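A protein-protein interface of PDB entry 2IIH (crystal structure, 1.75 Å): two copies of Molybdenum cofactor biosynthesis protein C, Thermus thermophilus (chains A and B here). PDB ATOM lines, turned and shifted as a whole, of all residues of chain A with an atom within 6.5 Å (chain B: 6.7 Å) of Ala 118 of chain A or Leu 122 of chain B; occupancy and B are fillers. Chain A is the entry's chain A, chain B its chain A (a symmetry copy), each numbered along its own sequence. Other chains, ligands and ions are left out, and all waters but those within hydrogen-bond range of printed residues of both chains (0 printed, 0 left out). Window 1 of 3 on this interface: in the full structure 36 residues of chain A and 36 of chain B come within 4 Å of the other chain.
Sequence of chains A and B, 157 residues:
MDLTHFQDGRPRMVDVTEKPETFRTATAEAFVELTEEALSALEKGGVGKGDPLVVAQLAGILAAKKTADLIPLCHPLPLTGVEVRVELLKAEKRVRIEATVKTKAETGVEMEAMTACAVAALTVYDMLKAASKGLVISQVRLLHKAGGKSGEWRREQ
The backbone carbonyl oxygen (O) of Ile 137 of chain B sits at hydrogen-bond distance from the backbone NH (N) of Val 140 of chain A. SD of Met 111 of chain A lies close to OD1 of Asp 126 of chain B.
The backbone carbonyl oxygen (O) of Met 111 of chain A is in hydrogen-bond range of the side-chain hydroxyl (OG1) of Thr 115 of chain A, at 2.7 Å. O of Val 119 of chain B is in hydrogen-bond range of OG1 of Thr 123 of chain B, at 2.9 Å.
Among the printed residues, merely in contact across the chains: Met 111 of chain A with Leu 122 of chain B (3.2 Å), Met 111 of chain A with Tyr 125 of chain B (3.5 Å), Ile 71 of chain A with Asp 126 of chain B (3.5 Å), Leu 70 of chain A with Val 119 of chain B (3.6 Å), Met 114 of chain A with Leu 122 of chain B (3.8 Å), Thr 115 of chain A with Leu 122 of chain B (3.8 Å), Leu 122 of chain A with Ala 118 of chain B (3.8 Å), Ala 118 of chain A with Leu 122 of chain B (3.8 Å) and Met 114 of chain A with Tyr 125 of chain B (3.9 Å).
Printed residues of chain B within 4 Å of Ala 118 of chain A: Leu 122 (3.8 Å). Leu 122 of chain B touches four residues of chain A. Printed residues of chain B within 4 Å of Met 111 of chain A: Leu 122, Tyr 125 and Asp 126. Of the printed residues of chain A, Ala 118 of chain B touches Leu 122. The nearest residue of chain B that does not touch Ala 118 of chain A is Ala 118 of chain B (4.9 Å). The nearest printed residue of chain A that does not touch Val 119 of chain B is Ile 71 of chain A (5.2 Å).
Of the 14 printed residues of chain B, 6 touch a printed residue of chain A. Printed residues of chain B that touch a printed residue of chain A: Ala 118, Val 119, Leu 122, Tyr 125, Asp 126 and Ile 137. Printed residues of chain A that touch a printed residue of chain B: Leu 70, Ile 71, Met 111, Met 114, Thr 115, Ala 118, Leu 122 and Val 140. Among the printed residues, 11 pairs touch across the chains. Among the printed residues, no Asp or Glu carboxylate lies within 4 Å of a Lys or Arg side-chain nitrogen of the other chain.
Ala 118 of chain A touches Leu 122 of chain B, and with the chains exchanged Leu 122 of chain A touches Ala 118 of chain B. 8 positions are printed for both chains. Of the 11 pairs that touch across the chains among the printed residues, 2 have their exchanged pair printed and touching as well.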
ATOM      1  N   GLU A  29     -11.288  -7.767 -28.080  1.00  0.00           N
ATOM      2  CA  GLU A  29     -11.453  -7.398 -29.476  1.00  0.00           C
ATOM      3  C   GLU A  29     -11.947  -8.595 -30.274  1.00  0.00           C
ATOM      4  O   GLU A  29     -11.862  -9.738 -29.821  1.00  0.00           O
ATOM      5  CB  GLU A  29     -10.130  -6.877 -30.056  1.00  0.00           C
ATOM      6  CG  GLU A  29      -9.219  -7.934 -30.644  1.00  0.00           C
ATOM      7  CD  GLU A  29      -7.852  -7.382 -31.021  1.00  0.00           C
ATOM      8  OE1 GLU A  29      -7.782  -6.239 -31.522  1.00  0.00           O
ATOM      9  OE2 GLU A  29      -6.852  -8.100 -30.824  1.00  0.00           O
ATOM     10  N   ALA A  30     -12.491  -8.312 -31.450  1.00  0.00           N
ATOM     11  CA  ALA A  30     -12.989  -9.334 -32.352  1.00  0.00           C
ATOM     12  C   ALA A  30     -12.796  -8.800 -33.760  1.00  0.00           C
ATOM     13  O   ALA A  30     -12.659  -7.592 -33.966  1.00  0.00           O
ATOM     14  CB  ALA A  30     -14.466  -9.610 -32.090  1.00  0.00           C
ATOM     15  N   LEU A  70     -26.681 -14.040 -20.342  1.00  0.00           N
ATOM     16  CA  LEU A  70     -26.250 -14.980 -21.387  1.00  0.00           C
ATOM     17  C   LEU A  70     -25.253 -16.034 -20.926  1.00  0.00           C
ATOM     18  O   LEU A  70     -25.257 -17.171 -21.415  1.00  0.00           O
ATOM     19  CB  LEU A  70     -25.635 -14.206 -22.557  1.00  0.00           C
ATOM     20  CG  LEU A  70     -26.521 -13.160 -23.234  1.00  0.00           C
ATOM     21  CD1 LEU A  70     -25.693 -12.363 -24.232  1.00  0.00           C
ATOM     22  CD2 LEU A  70     -27.688 -13.853 -23.928  1.00  0.00           C
ATOM     23  N   ILE A  71     -24.374 -15.648 -20.007  1.00  0.00           N
ATOM     24  CA  ILE A  71     -23.355 -16.548 -19.479  1.00  0.00           C
ATOM     25  C   ILE A  71     -23.858 -17.077 -18.131  1.00  0.00           C
ATOM     26  O   ILE A  71     -23.871 -16.356 -17.125  1.00  0.00           O
ATOM     27  CB  ILE A  71     -22.031 -15.785 -19.329  1.00  0.00           C
ATOM     28  CG1 ILE A  71     -21.708 -15.074 -20.652  1.00  0.00           C
ATOM     29  CG2 ILE A  71     -20.911 -16.734 -18.966  1.00  0.00           C
ATOM     30  CD1 ILE A  71     -20.492 -14.202 -20.578  1.00  0.00           C
ATOM     31  N   ILE A  97     -13.352  -4.826 -33.968  1.00  0.00           N
ATOM     32  CA  ILE A  97     -14.203  -4.413 -32.857  1.00  0.00           C
ATOM     33  C   ILE A  97     -13.385  -4.478 -31.569  1.00  0.00           C
ATOM     34  O   ILE A  97     -12.685  -5.458 -31.317  1.00  0.00           O
ATOM     35  CB  ILE A  97     -15.442  -5.339 -32.693  1.00  0.00           C
ATOM     36  CG1 ILE A  97     -16.278  -5.353 -33.978  1.00  0.00           C
ATOM     37  CG2 ILE A  97     -16.291  -4.859 -31.522  1.00  0.00           C
ATOM     38  CD1 ILE A  97     -15.766  -6.309 -35.048  1.00  0.00           C
ATOM     39  N   MET A 111     -15.846 -11.117 -19.139  1.00  0.00           N
ATOM     40  CA  MET A 111     -16.973 -11.623 -19.915  1.00  0.00           C
ATOM     41  C   MET A 111     -17.770 -10.513 -20.576  1.00  0.00           C
ATOM     42  O   MET A 111     -18.243 -10.674 -21.696  1.00  0.00           O
ATOM     43  CB  MET A 111     -17.898 -12.484 -19.049  1.00  0.00           C
ATOM     44  CG  MET A 111     -17.293 -13.809 -18.629  1.00  0.00           C
ATOM     45  SD  MET A 111     -16.309 -14.592 -19.944  1.00  0.00           S
ATOM     46  CE  MET A 111     -17.491 -14.765 -21.265  1.00  0.00           C
ATOM     47  N   ALA A 113     -16.610  -7.610 -21.623  1.00  0.00           N
ATOM     48  CA  ALA A 113     -15.843  -7.094 -22.757  1.00  0.00           C
ATOM     49  C   ALA A 113     -15.894  -8.083 -23.920  1.00  0.00           C
ATOM     50  O   ALA A 113     -16.116  -7.703 -25.071  1.00  0.00           O
ATOM     51  CB  ALA A 113     -14.391  -6.847 -22.344  1.00  0.00           C
ATOM     52  N   MET A 114     -15.692  -9.359 -23.612  1.00  0.00           N
ATOM     53  CA  MET A 114     -15.726 -10.409 -24.625  1.00  0.00           C
ATOM     54  C   MET A 114     -17.096 -10.508 -25.299  1.00  0.00           C
ATOM     55  O   MET A 114     -17.184 -10.628 -26.519  1.00  0.00           O
ATOM     56  CB  MET A 114     -15.374 -11.761 -23.995  1.00  0.00           C
ATOM     57  CG  MET A 114     -13.918 -11.916 -23.574  1.00  0.00           C
ATOM     58  SD  MET A 114     -12.812 -12.137 -24.983  1.00  0.00           S
ATOM     59  CE  MET A 114     -13.018 -13.914 -25.306  1.00  0.00           C
ATOM     60  N   THR A 115     -18.160 -10.451 -24.505  1.00  0.00           N
ATOM     61  CA  THR A 115     -19.512 -10.558 -25.042  1.00  0.00           C
ATOM     62  C   THR A 115     -19.881  -9.350 -25.901  1.00  0.00           C
ATOM     63  O   THR A 115     -20.560  -9.487 -26.913  1.00  0.00           O
ATOM     64  CB  THR A 115     -20.542 -10.727 -23.905  1.00  0.00           C
ATOM     65  OG1 THR A 115     -20.210 -11.894 -23.139  1.00  0.00           O
ATOM     66  CG2 THR A 115     -21.947 -10.888 -24.474  1.00  0.00           C
ATOM     67  N   ALA A 116     -19.437  -8.168 -25.491  1.00  0.00           N
ATOM     68  CA  ALA A 116     -19.704  -6.959 -26.254  1.00  0.00           C
ATOM     69  C   ALA A 116     -19.090  -7.100 -27.652  1.00  0.00           C
ATOM     70  O   ALA A 116     -19.721  -6.776 -28.655  1.00  0.00           O
ATOM     71  CB  ALA A 116     -19.110  -5.745 -25.534  1.00  0.00           C
ATOM     72  N   CYS A 117     -17.857  -7.597 -27.717  1.00  0.00           N
ATOM     73  CA  CYS A 117     -17.195  -7.765 -29.007  1.00  0.00           C
ATOM     74  C   CYS A 117     -17.870  -8.832 -29.851  1.00  0.00           C
ATOM     75  O   CYS A 117     -18.058  -8.648 -31.054  1.00  0.00           O
ATOM     76  CB  CYS A 117     -15.721  -8.126 -28.817  1.00  0.00           C
ATOM     77  SG  CYS A 117     -14.733  -6.758 -28.188  1.00  0.00           S
ATOM     78  N   ALA A 118     -18.244  -9.940 -29.213  1.00  0.00           N
ATOM     79  CA  ALA A 118     -18.895 -11.043 -29.910  1.00  0.00           C
ATOM     80  C   ALA A 118     -20.220 -10.649 -30.537  1.00  0.00           C
ATOM     81  O   ALA A 118     -20.488 -10.983 -31.690  1.00  0.00           O
ATOM     82  CB  ALA A 118     -19.106 -12.218 -28.960  1.00  0.00           C
ATOM     83  N   VAL A 119     -21.055  -9.941 -29.782  1.00  0.00           N
ATOM     84  CA  VAL A 119     -22.353  -9.527 -30.301  1.00  0.00           C
ATOM     85  C   VAL A 119     -22.221  -8.427 -31.354  1.00  0.00           C
ATOM     86  O   VAL A 119     -22.991  -8.382 -32.310  1.00  0.00           O
ATOM     87  CB  VAL A 119     -23.293  -9.081 -29.148  1.00  0.00           C
ATOM     88  CG1 VAL A 119     -24.606  -8.552 -29.714  1.00  0.00           C
ATOM     89  CG2 VAL A 119     -23.573 -10.275 -28.232  1.00  0.00           C
ATOM     90  N   ALA A 120     -21.241  -7.542 -31.200  1.00  0.00           N
ATOM     91  CA  ALA A 120     -21.049  -6.495 -32.196  1.00  0.00           C
ATOM     92  C   ALA A 120     -20.653  -7.191 -33.499  1.00  0.00           C
ATOM     93  O   ALA A 120     -21.142  -6.850 -34.576  1.00  0.00           O
ATOM     94  CB  ALA A 120     -19.956  -5.526 -31.747  1.00  0.00           C
ATOM     95  N   ALA A 121     -19.775  -8.188 -33.394  1.00  0.00           N
ATOM     96  CA  ALA A 121     -19.340  -8.929 -34.575  1.00  0.00           C
ATOM     97  C   ALA A 121     -20.534  -9.646 -35.208  1.00  0.00           C
ATOM     98  O   ALA A 121     -20.694  -9.633 -36.425  1.00  0.00           O
ATOM     99  CB  ALA A 121     -18.246  -9.932 -34.201  1.00  0.00           C
ATOM    100  N   LEU A 122     -21.377 -10.263 -34.382  1.00  0.00           N
ATOM    101  CA  LEU A 122     -22.558 -10.962 -34.892  1.00  0.00           C
ATOM    102  C   LEU A 122     -23.490  -9.993 -35.607  1.00  0.00           C
ATOM    103  O   LEU A 122     -24.168 -10.363 -36.568  1.00  0.00           O
ATOM    104  CB  LEU A 122     -23.314 -11.650 -33.744  1.00  0.00           C
ATOM    105  CG  LEU A 122     -22.687 -12.914 -33.149  1.00  0.00           C
ATOM    106  CD1 LEU A 122     -23.358 -13.245 -31.821  1.00  0.00           C
ATOM    107  CD2 LEU A 122     -22.850 -14.077 -34.123  1.00  0.00           C
ATOM    108  N   THR A 123     -23.524  -8.747 -35.143  1.00  0.00           N
ATOM    109  CA  THR A 123     -24.386  -7.747 -35.761  1.00  0.00           C
ATOM    110  C   THR A 123     -23.824  -7.304 -37.102  1.00  0.00           C
ATOM    111  O   THR A 123     -24.573  -7.066 -38.050  1.00  0.00           O
ATOM    112  CB  THR A 123     -24.579  -6.557 -34.822  1.00  0.00           C
ATOM    113  OG1 THR A 123     -25.194  -7.028 -33.618  1.00  0.00           O
ATOM    114  CG2 THR A 123     -25.473  -5.502 -35.460  1.00  0.00           C
ATOM    115  N   ILE A 137     -16.305 -14.692 -38.381  1.00  0.00           N
ATOM    116  CA  ILE A 137     -15.979 -13.908 -37.195  1.00  0.00           C
ATOM    117  C   ILE A 137     -14.739 -14.590 -36.639  1.00  0.00           C
ATOM    118  O   ILE A 137     -14.771 -15.772 -36.301  1.00  0.00           O
ATOM    119  CB  ILE A 137     -17.068 -13.978 -36.115  1.00  0.00           C
ATOM    120  CG1 ILE A 137     -18.351 -13.331 -36.638  1.00  0.00           C
ATOM    121  CG2 ILE A 137     -16.549 -13.323 -34.839  1.00  0.00           C
ATOM    122  CD1 ILE A 137     -18.245 -11.881 -36.938  1.00  0.00           C
ATOM    123  N   VAL A 140     -12.002 -13.656 -31.324  1.00  0.00           N
ATOM    124  CA  VAL A 140     -12.619 -12.913 -30.225  1.00  0.00           C
ATOM    125  C   VAL A 140     -11.654 -13.247 -29.097  1.00  0.00           C
ATOM    126  O   VAL A 140     -11.507 -14.413 -28.728  1.00  0.00           O
ATOM    127  CB  VAL A 140     -14.014 -13.443 -29.857  1.00  0.00           C
ATOM    128  CG1 VAL A 140     -14.618 -12.567 -28.772  1.00  0.00           C
ATOM    129  CG2 VAL A 140     -14.907 -13.471 -31.095  1.00  0.00           C
ATOM    130  N   VAL B  32     -12.805 -22.933 -29.931  1.00  0.00           N
ATOM    131  CA  VAL B  32     -12.073 -22.310 -28.837  1.00  0.00           C
ATOM    132  C   VAL B  32     -10.725 -23.014 -28.867  1.00  0.00           C
ATOM    133  O   VAL B  32     -10.668 -24.242 -28.751  1.00  0.00           O
ATOM    134  CB  VAL B  32     -12.720 -22.563 -27.461  1.00  0.00           C
ATOM    135  CG1 VAL B  32     -11.994 -21.742 -26.401  1.00  0.00           C
ATOM    136  CG2 VAL B  32     -14.195 -22.206 -27.500  1.00  0.00           C
ATOM    137  N   ALA B  56     -21.781 -24.857 -21.332  1.00  0.00           N
ATOM    138  CA  ALA B  56     -21.734 -24.132 -22.600  1.00  0.00           C
ATOM    139  C   ALA B  56     -22.796 -24.604 -23.588  1.00  0.00           C
ATOM    140  O   ALA B  56     -23.380 -23.802 -24.318  1.00  0.00           O
ATOM    141  CB  ALA B  56     -20.339 -24.275 -23.226  1.00  0.00           C
ATOM    142  N   CYS B 117     -23.675 -20.557 -31.272  1.00  0.00           N
ATOM    143  CA  CYS B 117     -22.274 -20.968 -31.246  1.00  0.00           C
ATOM    144  C   CYS B 117     -21.404 -19.956 -30.520  1.00  0.00           C
ATOM    145  O   CYS B 117     -20.533 -20.331 -29.736  1.00  0.00           O
ATOM    146  CB  CYS B 117     -21.741 -21.170 -32.665  1.00  0.00           C
ATOM    147  SG  CYS B 117     -22.428 -22.623 -33.478  1.00  0.00           S
ATOM    148  N   ALA B 118     -21.654 -18.672 -30.777  1.00  0.00           N
ATOM    149  CA  ALA B 118     -20.885 -17.602 -30.151  1.00  0.00           C
ATOM    150  C   ALA B 118     -21.007 -17.590 -28.638  1.00  0.00           C
ATOM    151  O   ALA B 118     -20.008 -17.461 -27.934  1.00  0.00           O
ATOM    152  CB  ALA B 118     -21.311 -16.249 -30.712  1.00  0.00           C
ATOM    153  N   VAL B 119     -22.230 -17.720 -28.134  1.00  0.00           N
ATOM    154  CA  VAL B 119     -22.440 -17.710 -26.691  1.00  0.00           C
ATOM    155  C   VAL B 119     -21.929 -18.991 -26.032  1.00  0.00           C
ATOM    156  O   VAL B 119     -21.430 -18.959 -24.910  1.00  0.00           O
ATOM    157  CB  VAL B 119     -23.937 -17.472 -26.352  1.00  0.00           C
ATOM    158  CG1 VAL B 119     -24.157 -17.570 -24.846  1.00  0.00           C
ATOM    159  CG2 VAL B 119     -24.352 -16.083 -26.842  1.00  0.00           C
ATOM    160  N   ALA B 120     -22.033 -20.122 -26.723  1.00  0.00           N
ATOM    161  CA  ALA B 120     -21.526 -21.365 -26.154  1.00  0.00           C
ATOM    162  C   ALA B 120     -20.010 -21.206 -26.022  1.00  0.00           C
ATOM    163  O   ALA B 120     -19.418 -21.576 -25.008  1.00  0.00           O
ATOM    164  CB  ALA B 120     -21.868 -22.546 -27.064  1.00  0.00           C
ATOM    165  N   ALA B 121     -19.384 -20.632 -27.048  1.00  0.00           N
ATOM    166  CA  ALA B 121     -17.939 -20.419 -27.018  1.00  0.00           C
ATOM    167  C   ALA B 121     -17.578 -19.468 -25.875  1.00  0.00           C
ATOM    168  O   ALA B 121     -16.617 -19.706 -25.149  1.00  0.00           O
ATOM    169  CB  ALA B 121     -17.456 -19.859 -28.359  1.00  0.00           C
ATOM    170  N   LEU B 122     -18.352 -18.397 -25.711  1.00  0.00           N
ATOM    171  CA  LEU B 122     -18.095 -17.438 -24.635  1.00  0.00           C
ATOM    172  C   LEU B 122     -18.218 -18.111 -23.274  1.00  0.00           C
ATOM    173  O   LEU B 122     -17.520 -17.746 -22.325  1.00  0.00           O
ATOM    174  CB  LEU B 122     -19.081 -16.261 -24.717  1.00  0.00           C
ATOM    175  CG  LEU B 122     -18.858 -15.235 -25.831  1.00  0.00           C
ATOM    176  CD1 LEU B 122     -20.101 -14.367 -25.987  1.00  0.00           C
ATOM    177  CD2 LEU B 122     -17.649 -14.366 -25.498  1.00  0.00           C
ATOM    178  N   THR B 123     -19.103 -19.098 -23.175  1.00  0.00           N
ATOM    179  CA  THR B 123     -19.292 -19.803 -21.914  1.00  0.00           C
ATOM    180  C   THR B 123     -18.122 -20.732 -21.633  1.00  0.00           C
ATOM    181  O   THR B 123     -17.697 -20.879 -20.487  1.00  0.00           O
ATOM    182  CB  THR B 123     -20.615 -20.567 -21.924  1.00  0.00           C
ATOM    183  OG1 THR B 123     -21.679 -19.625 -22.100  1.00  0.00           O
ATOM    184  CG2 THR B 123     -20.821 -21.314 -20.613  1.00  0.00           C
ATOM    185  N   VAL B 124     -17.589 -21.352 -22.680  1.00  0.00           N
ATOM    186  CA  VAL B 124     -16.428 -22.216 -22.511  1.00  0.00           C
ATOM    187  C   VAL B 124     -15.300 -21.324 -21.986  1.00  0.00           C
ATOM    188  O   VAL B 124     -14.586 -21.686 -21.050  1.00  0.00           O
ATOM    189  CB  VAL B 124     -16.003 -22.852 -23.853  1.00  0.00           C
ATOM    190  CG1 VAL B 124     -14.636 -23.527 -23.706  1.00  0.00           C
ATOM    191  CG2 VAL B 124     -17.050 -23.865 -24.300  1.00  0.00           C
ATOM    192  N   TYR B 125     -15.153 -20.146 -22.589  1.00  0.00           N
ATOM    193  CA  TYR B 125     -14.123 -19.199 -22.170  1.00  0.00           C
ATOM    194  C   TYR B 125     -14.333 -18.796 -20.713  1.00  0.00           C
ATOM    195  O   TYR B 125     -13.392 -18.780 -19.916  1.00  0.00           O
ATOM    196  CB  TYR B 125     -14.162 -17.935 -23.044  1.00  0.00           C
ATOM    197  CG  TYR B 125     -13.180 -16.870 -22.604  1.00  0.00           C
ATOM    198  CD1 TYR B 125     -11.826 -16.969 -22.921  1.00  0.00           C
ATOM    199  CD2 TYR B 125     -13.594 -15.794 -21.816  1.00  0.00           C
ATOM    200  CE1 TYR B 125     -10.907 -16.020 -22.463  1.00  0.00           C
ATOM    201  CE2 TYR B 125     -12.683 -14.842 -21.353  1.00  0.00           C
ATOM    202  CZ  TYR B 125     -11.341 -14.965 -21.678  1.00  0.00           C
ATOM    203  OH  TYR B 125     -10.434 -14.045 -21.202  1.00  0.00           O
ATOM    204  N   ASP B 126     -15.575 -18.469 -20.361  1.00  0.00           N
ATOM    205  CA  ASP B 126     -15.877 -18.048 -18.996  1.00  0.00           C
ATOM    206  C   ASP B 126     -15.411 -19.042 -17.947  1.00  0.00           C
ATOM    207  O   ASP B 126     -14.872 -18.661 -16.911  1.00  0.00           O
ATOM    208  CB  ASP B 126     -17.381 -17.823 -18.811  1.00  0.00           C
ATOM    209  CG  ASP B 126     -17.743 -17.485 -17.369  1.00  0.00           C
ATOM    210  OD1 ASP B 126     -17.185 -16.505 -16.839  1.00  0.00           O
ATOM    211  OD2 ASP B 126     -18.575 -18.200 -16.765  1.00  0.00           O
ATOM    212  N   MET B 127     -15.603 -20.321 -18.222  1.00  0.00           N
ATOM    213  CA  MET B 127     -15.229 -21.328 -17.246  1.00  0.00           C
ATOM    214  C   MET B 127     -13.810 -21.872 -17.308  1.00  0.00           C
ATOM    215  O   MET B 127     -13.452 -22.755 -16.534  1.00  0.00           O
ATOM    216  CB  MET B 127     -16.253 -22.446 -17.294  1.00  0.00           C
ATOM    217  CG  MET B 127     -17.596 -21.954 -16.785  1.00  0.00           C
ATOM    218  SD  MET B 127     -18.908 -23.071 -17.132  1.00  0.00           S
ATOM    219  CE  MET B 127     -18.522 -24.386 -15.985  1.00  0.00           C
ATOM    220  N   ILE B 137     -11.367 -17.354 -29.096  1.00  0.00           N
ATOM    221  CA  ILE B 137     -12.546 -17.899 -29.760  1.00  0.00           C
ATOM    222  C   ILE B 137     -12.285 -17.639 -31.235  1.00  0.00           C
ATOM    223  O   ILE B 137     -12.125 -16.492 -31.651  1.00  0.00           O
ATOM    224  CB  ILE B 137     -13.838 -17.159 -29.381  1.00  0.00           C
ATOM    225  CG1 ILE B 137     -14.129 -17.364 -27.894  1.00  0.00           C
ATOM    226  CG2 ILE B 137     -14.971 -17.642 -30.281  1.00  0.00           C
ATOM    227  CD1 ILE B 137     -14.397 -18.769 -27.496  1.00  0.00           C
